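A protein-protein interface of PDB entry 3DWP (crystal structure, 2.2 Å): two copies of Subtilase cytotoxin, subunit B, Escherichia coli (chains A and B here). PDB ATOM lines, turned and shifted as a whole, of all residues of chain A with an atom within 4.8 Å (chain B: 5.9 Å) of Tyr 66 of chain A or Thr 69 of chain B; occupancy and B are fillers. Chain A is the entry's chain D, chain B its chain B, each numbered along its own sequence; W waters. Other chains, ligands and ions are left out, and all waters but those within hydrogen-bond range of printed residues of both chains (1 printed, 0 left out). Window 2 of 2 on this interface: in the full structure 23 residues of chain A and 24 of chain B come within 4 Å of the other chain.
Water W1 lies within hydrogen-bond range of the side-chain hydroxyl (OH) of Tyr 61 of chain B (3.1 Å) and the backbone carbonyl oxygen (O) of Asn 62 of chain A (3.3 Å).
The side-chain hydroxyl (OH) of Tyr 61 of chain B is in hydrogen-bond range of the side-chain amide oxygen (OE1) of Gln 63 of chain A.
The side-chain hydroxyl (OH) of Tyr 68 of chain B lies within hydrogen-bond range of the side-chain amide oxygen (OE1) of Gln 72 of chain A, at 2.7 Å.
The side-chain hydroxyl (OG1) of Thr 69 of chain B lies within hydrogen-bond range of the side-chain hydroxyl (OH) of Tyr 66 of chain A, 2.5 Å away.
Tyr 66 of chain A touches Leu 65 of chain B, but with the chains exchanged Leu 65 of chain A does not touch Tyr 66 of chain B (12.4 Å).
Tyr 66 of chain A touches Tyr 68 of chain B, but with the chains exchanged Tyr 68 of chain A does not touch Tyr 66 of chain B (14.2 Å).
Tyr 66 of chain A touches Thr 69 of chain B, but with the chains exchanged Thr 69 of chain A does not touch Tyr 66 of chain B (12.6 Å).
Of the 7 pairs that touch across the chains among the printed residues, none has its exchanged pair printed and touching as well.
Tyr 66 of chain A touches just these residues of chain B: Leu 65, Tyr 68 and Thr 69.
Thr 69 of chain B touches just one residue of chain A: Tyr 66.
Printed residues of chain B within 4 Å of Gln 63 of chain A: Tyr 61 and Leu 65.
Printed residues of chain B within 4 Å of Gln 72 of chain A: Tyr 68.
Printed residues of chain B within 4 Å of Asn 62 of chain A: Tyr 61 (3.7 Å).
Printed residues of chain A within 4 Å of Tyr 61 of chain B: Asn 62 and Gln 63.
The nearest residue of chain B that does not touch Tyr 66 of chain A is Tyr 61 of chain B (5.8 Å).
The side-chain hydroxyl of Thr 69 of chain B lies within hydrogen-bond range of the backbone carbonyl oxygen of Leu 65 of chain B (2.6 Å).
The side-chain amide nitrogen of Gln 72 of chain A is in hydrogen-bond range of the side-chain hydroxyl of Thr 70 of chain A, 2.5 Å away.
Of the 9 printed residues of chain B, 4 touch a printed residue of chain A.
Of the 10 printed residues of chain A, 4 touch a printed residue of chain B.
Hydrophobic or aromatic side chains of chain A that line the printed part of chain B: Tyr 66.
Among the printed residues, 7 pairs touch across the chains.
Among the printed residues, no Asp or Glu carboxylate lies within 4 Å of a Lys or Arg side-chain nitrogen of the other chain.
Asn 62 of chain A touches Tyr 61 of chain B (CB to OH, 3.7 Å).
Leu 65 of chain B touches Gln 63 of chain A.
Tyr 66 of chain A touches Leu 65 of chain B (CD1 to CD2, 3.9 Å).
Tyr 68 of chain B touches Tyr 66 of chain A.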
ATOM      1  N   ASN A  62      27.163  -4.329  16.853  1.00  0.00           N
ATOM      2  CA  ASN A  62      25.892  -3.919  17.406  1.00  0.00           C
ATOM      3  C   ASN A  62      25.983  -3.131  18.717  1.00  0.00           C
ATOM      4  O   ASN A  62      25.341  -2.102  18.881  1.00  0.00           O
ATOM      5  CB  ASN A  62      25.041  -5.179  17.639  1.00  0.00           C
ATOM      6  CG  ASN A  62      24.280  -5.644  16.396  1.00  0.00           C
ATOM      7  OD1 ASN A  62      24.222  -4.968  15.341  1.00  0.00           O
ATOM      8  ND2 ASN A  62      23.661  -6.826  16.527  1.00  0.00           N
ATOM      9  N   GLN A  63      26.776  -3.627  19.657  1.00  0.00           N
ATOM     10  CA  GLN A  63      26.865  -3.040  20.970  1.00  0.00           C
ATOM     11  C   GLN A  63      27.704  -1.755  20.965  1.00  0.00           C
ATOM     12  O   GLN A  63      27.380  -0.791  21.670  1.00  0.00           O
ATOM     13  CB  GLN A  63      27.434  -4.061  21.960  1.00  0.00           C
ATOM     14  CG  GLN A  63      27.213  -3.702  23.425  1.00  0.00           C
ATOM     15  CD  GLN A  63      25.738  -3.636  23.809  1.00  0.00           C
ATOM     16  OE1 GLN A  63      24.973  -4.532  23.496  1.00  0.00           O
ATOM     17  NE2 GLN A  63      25.342  -2.569  24.487  1.00  0.00           N
ATOM     18  N   ALA A  64      28.781  -1.778  20.186  1.00  0.00           N
ATOM     19  CA  ALA A  64      29.637  -0.615  19.932  1.00  0.00           C
ATOM     20  C   ALA A  64      28.867   0.541  19.283  1.00  0.00           C
ATOM     21  O   ALA A  64      28.932   1.655  19.776  1.00  0.00           O
ATOM     22  CB  ALA A  64      30.858  -1.010  19.064  1.00  0.00           C
ATOM     23  N   LEU A  65      28.125   0.261  18.209  1.00  0.00           N
ATOM     24  CA  LEU A  65      27.277   1.262  17.574  1.00  0.00           C
ATOM     25  C   LEU A  65      26.168   1.808  18.502  1.00  0.00           C
ATOM     26  O   LEU A  65      25.873   3.014  18.465  1.00  0.00           O
ATOM     27  CB  LEU A  65      26.684   0.728  16.258  1.00  0.00           C
ATOM     28  CG  LEU A  65      25.966   1.760  15.358  1.00  0.00           C
ATOM     29  CD1 LEU A  65      26.954   2.833  14.870  1.00  0.00           C
ATOM     30  CD2 LEU A  65      25.276   1.106  14.210  1.00  0.00           C
ATOM     31  N   TYR A  66      25.561   0.928  19.316  1.00  0.00           N
ATOM     32  CA  TYR A  66      24.631   1.349  20.379  1.00  0.00           C
ATOM     33  C   TYR A  66      25.254   2.388  21.325  1.00  0.00           C
ATOM     34  O   TYR A  66      24.671   3.440  21.537  1.00  0.00           O
ATOM     35  CB  TYR A  66      24.120   0.139  21.194  1.00  0.00           C
ATOM     36  CG  TYR A  66      23.140   0.514  22.282  1.00  0.00           C
ATOM     37  CD1 TYR A  66      21.777   0.611  22.004  1.00  0.00           C
ATOM     38  CD2 TYR A  66      23.583   0.799  23.591  1.00  0.00           C
ATOM     39  CE1 TYR A  66      20.862   0.965  22.991  1.00  0.00           C
ATOM     40  CE2 TYR A  66      22.685   1.161  24.596  1.00  0.00           C
ATOM     41  CZ  TYR A  66      21.319   1.238  24.282  1.00  0.00           C
ATOM     42  OH  TYR A  66      20.415   1.606  25.248  1.00  0.00           O
ATOM     43  N   PHE A  67      26.420   2.065  21.897  1.00  0.00           N
ATOM     44  CA  PHE A  67      27.116   2.924  22.855  1.00  0.00           C
ATOM     45  C   PHE A  67      27.686   4.189  22.206  1.00  0.00           C
ATOM     46  O   PHE A  67      27.831   5.231  22.865  1.00  0.00           O
ATOM     47  CB  PHE A  67      28.292   2.186  23.505  1.00  0.00           C
ATOM     48  CG  PHE A  67      27.911   1.086  24.487  1.00  0.00           C
ATOM     49  CD1 PHE A  67      26.836   1.222  25.370  1.00  0.00           C
ATOM     50  CD2 PHE A  67      28.696  -0.071  24.576  1.00  0.00           C
ATOM     51  CE1 PHE A  67      26.531   0.212  26.295  1.00  0.00           C
ATOM     52  CE2 PHE A  67      28.389  -1.073  25.517  1.00  0.00           C
ATOM     53  CZ  PHE A  67      27.296  -0.924  26.358  1.00  0.00           C
ATOM     54  N   TYR A  68      28.081   4.086  20.941  1.00  0.00           N
ATOM     55  CA  TYR A  68      28.469   5.275  20.175  1.00  0.00           C
ATOM     56  C   TYR A  68      27.264   6.235  20.059  1.00  0.00           C
ATOM     57  O   TYR A  68      27.407   7.449  20.183  1.00  0.00           O
ATOM     58  CB  TYR A  68      29.003   4.892  18.791  1.00  0.00           C
ATOM     59  CG  TYR A  68      29.179   6.104  17.915  1.00  0.00           C
ATOM     60  CD1 TYR A  68      30.243   6.987  18.131  1.00  0.00           C
ATOM     61  CD2 TYR A  68      28.254   6.400  16.904  1.00  0.00           C
ATOM     62  CE1 TYR A  68      30.388   8.125  17.367  1.00  0.00           C
ATOM     63  CE2 TYR A  68      28.397   7.526  16.127  1.00  0.00           C
ATOM     64  CZ  TYR A  68      29.469   8.380  16.358  1.00  0.00           C
ATOM     65  OH  TYR A  68      29.622   9.493  15.592  1.00  0.00           O
ATOM     66  N   THR A  69      26.077   5.663  19.863  1.00  0.00           N
ATOM     67  CA  THR A  69      24.821   6.425  19.828  1.00  0.00           C
ATOM     68  C   THR A  69      24.452   7.130  21.149  1.00  0.00           C
ATOM     69  O   THR A  69      24.181   8.345  21.143  1.00  0.00           O
ATOM     70  CB  THR A  69      23.649   5.544  19.329  1.00  0.00           C
ATOM     71  OG1 THR A  69      24.054   4.872  18.131  1.00  0.00           O
ATOM     72  CG2 THR A  69      22.370   6.375  19.094  1.00  0.00           C
ATOM     73  N   THR A  70      24.442   6.391  22.265  1.00  0.00           N
ATOM     74  CA  THR A  70      24.114   6.981  23.577  1.00  0.00           C
ATOM     75  C   THR A  70      25.200   7.920  24.105  1.00  0.00           C
ATOM     76  O   THR A  70      24.901   8.910  24.797  1.00  0.00           O
ATOM     77  CB  THR A  70      23.761   5.919  24.654  1.00  0.00           C
ATOM     78  OG1 THR A  70      24.926   5.163  25.000  1.00  0.00           O
ATOM     79  CG2 THR A  70      22.708   4.954  24.115  1.00  0.00           C
ATOM     80  N   GLN A  72      27.411   7.141  26.283  1.00  0.00           N
ATOM     81  CA  GLN A  72      27.668   6.806  27.684  1.00  0.00           C
ATOM     82  C   GLN A  72      29.080   6.236  27.836  1.00  0.00           C
ATOM     83  O   GLN A  72      29.594   5.639  26.897  1.00  0.00           O
ATOM     84  CB  GLN A  72      26.621   5.788  28.179  1.00  0.00           C
ATOM     85  CG  GLN A  72      26.769   4.342  27.637  1.00  0.00           C
ATOM     86  CD  GLN A  72      25.515   3.522  27.869  1.00  0.00           C
ATOM     87  OE1 GLN A  72      25.372   2.834  28.882  1.00  0.00           O
ATOM     88  NE2 GLN A  72      24.586   3.622  26.949  1.00  0.00           N
ATOM     89  N   TYR B  61      19.137 -11.217  23.403  1.00  0.00           N
ATOM     90  CA  TYR B  61      20.055 -10.070  23.247  1.00  0.00           C
ATOM     91  C   TYR B  61      19.274  -8.828  22.853  1.00  0.00           C
ATOM     92  O   TYR B  61      19.377  -7.800  23.505  1.00  0.00           O
ATOM     93  CB  TYR B  61      21.184 -10.342  22.236  1.00  0.00           C
ATOM     94  CG  TYR B  61      22.011  -9.111  21.955  1.00  0.00           C
ATOM     95  CD1 TYR B  61      22.938  -8.630  22.896  1.00  0.00           C
ATOM     96  CD2 TYR B  61      21.860  -8.402  20.756  1.00  0.00           C
ATOM     97  CE1 TYR B  61      23.691  -7.481  22.663  1.00  0.00           C
ATOM     98  CE2 TYR B  61      22.627  -7.264  20.505  1.00  0.00           C
ATOM     99  CZ  TYR B  61      23.530  -6.810  21.467  1.00  0.00           C
ATOM    100  OH  TYR B  61      24.263  -5.693  21.210  1.00  0.00           O
ATOM    101  N   ALA B  64      16.701  -7.841  25.653  1.00  0.00           N
ATOM    102  CA  ALA B  64      17.382  -7.247  26.804  1.00  0.00           C
ATOM    103  C   ALA B  64      17.919  -5.839  26.516  1.00  0.00           C
ATOM    104  O   ALA B  64      17.825  -4.969  27.379  1.00  0.00           O
ATOM    105  CB  ALA B  64      18.506  -8.155  27.333  1.00  0.00           C
ATOM    106  N   LEU B  65      18.501  -5.630  25.336  1.00  0.00           N
ATOM    107  CA  LEU B  65      19.006  -4.331  24.951  1.00  0.00           C
ATOM    108  C   LEU B  65      17.870  -3.323  24.810  1.00  0.00           C
ATOM    109  O   LEU B  65      17.996  -2.145  25.209  1.00  0.00           O
ATOM    110  CB  LEU B  65      19.871  -4.406  23.667  1.00  0.00           C
ATOM    111  CG  LEU B  65      20.582  -3.100  23.286  1.00  0.00           C
ATOM    112  CD1 LEU B  65      21.529  -2.642  24.384  1.00  0.00           C
ATOM    113  CD2 LEU B  65      21.312  -3.221  21.951  1.00  0.00           C
ATOM    114  N   TYR B  66      16.763  -3.783  24.238  1.00  0.00           N
ATOM    115  CA  TYR B  66      15.531  -3.003  24.182  1.00  0.00           C
ATOM    116  C   TYR B  66      15.101  -2.521  25.578  1.00  0.00           C
ATOM    117  O   TYR B  66      14.888  -1.322  25.779  1.00  0.00           O
ATOM    118  CB  TYR B  66      14.422  -3.835  23.528  1.00  0.00           C
ATOM    119  CG  TYR B  66      13.141  -3.075  23.333  1.00  0.00           C
ATOM    120  CD1 TYR B  66      12.929  -2.311  22.181  1.00  0.00           C
ATOM    121  CD2 TYR B  66      12.140  -3.096  24.318  1.00  0.00           C
ATOM    122  CE1 TYR B  66      11.748  -1.590  22.010  1.00  0.00           C
ATOM    123  CE2 TYR B  66      10.974  -2.401  24.151  1.00  0.00           C
ATOM    124  CZ  TYR B  66      10.781  -1.645  22.993  1.00  0.00           C
ATOM    125  OH  TYR B  66       9.593  -0.959  22.826  1.00  0.00           O
ATOM    126  N   PHE B  67      14.982  -3.460  26.531  1.00  0.00           N
ATOM    127  CA  PHE B  67      14.519  -3.151  27.884  1.00  0.00           C
ATOM    128  C   PHE B  67      15.533  -2.341  28.715  1.00  0.00           C
ATOM    129  O   PHE B  67      15.146  -1.527  29.557  1.00  0.00           O
ATOM    130  CB  PHE B  67      14.149  -4.424  28.657  1.00  0.00           C
ATOM    131  CG  PHE B  67      12.887  -5.103  28.188  1.00  0.00           C
ATOM    132  CD1 PHE B  67      11.769  -4.366  27.798  1.00  0.00           C
ATOM    133  CD2 PHE B  67      12.806  -6.501  28.187  1.00  0.00           C
ATOM    134  CE1 PHE B  67      10.589  -5.007  27.410  1.00  0.00           C
ATOM    135  CE2 PHE B  67      11.649  -7.159  27.803  1.00  0.00           C
ATOM    136  CZ  PHE B  67      10.527  -6.417  27.423  1.00  0.00           C
ATOM    137  N   TYR B  68      16.821  -2.589  28.512  1.00  0.00           N
ATOM    138  CA  TYR B  68      17.858  -1.723  29.068  1.00  0.00           C
ATOM    139  C   TYR B  68      17.679  -0.272  28.619  1.00  0.00           C
ATOM    140  O   TYR B  68      17.897   0.646  29.389  1.00  0.00           O
ATOM    141  CB  TYR B  68      19.260  -2.200  28.664  1.00  0.00           C
ATOM    142  CG  TYR B  68      20.349  -1.201  29.049  1.00  0.00           C
ATOM    143  CD1 TYR B  68      20.787  -1.077  30.385  1.00  0.00           C
ATOM    144  CD2 TYR B  68      20.911  -0.356  28.095  1.00  0.00           C
ATOM    145  CE1 TYR B  68      21.754  -0.152  30.744  1.00  0.00           C
ATOM    146  CE2 TYR B  68      21.885   0.579  28.447  1.00  0.00           C
ATOM    147  CZ  TYR B  68      22.296   0.673  29.771  1.00  0.00           C
ATOM    148  OH  TYR B  68      23.270   1.589  30.098  1.00  0.00           O
ATOM    149  N   THR B  69      17.317  -0.091  27.355  1.00  0.00           N
ATOM    150  CA  THR B  69      17.108   1.208  26.738  1.00  0.00           C
ATOM    151  C   THR B  69      15.868   1.934  27.284  1.00  0.00           C
ATOM    152  O   THR B  69      15.925   3.123  27.551  1.00  0.00           O
ATOM    153  CB  THR B  69      17.025   1.029  25.163  1.00  0.00           C
ATOM    154  OG1 THR B  69      18.243   0.436  24.697  1.00  0.00           O
ATOM    155  CG2 THR B  69      16.766   2.353  24.410  1.00  0.00           C
ATOM    156  N   THR B  70      14.745   1.246  27.413  1.00  0.00           N
ATOM    157  CA  THR B  70      13.525   1.893  27.902  1.00  0.00           C
ATOM    158  C   THR B  70      13.517   2.100  29.410  1.00  0.00           C
ATOM    159  O   THR B  70      12.856   3.017  29.880  1.00  0.00           O
ATOM    160  CB  THR B  70      12.211   1.167  27.505  1.00  0.00           C
ATOM    161  OG1 THR B  70      12.185  -0.142  28.090  1.00  0.00           O
ATOM    162  CG2 THR B  70      12.024   1.091  25.974  1.00  0.00           C
ATOM    163  N   GLY B  71      14.223   1.234  30.148  1.00  0.00           N
ATOM    164  CA  GLY B  71      14.260   1.273  31.602  1.00  0.00           C
ATOM    165  C   GLY B  71      12.987   0.800  32.294  1.00  0.00           C
ATOM    166  O   GLY B  71      12.805   1.009  33.509  1.00  0.00           O
HETATM  167  O   HOH W   1      22.687  -4.134  18.976  1.00  0.00           O
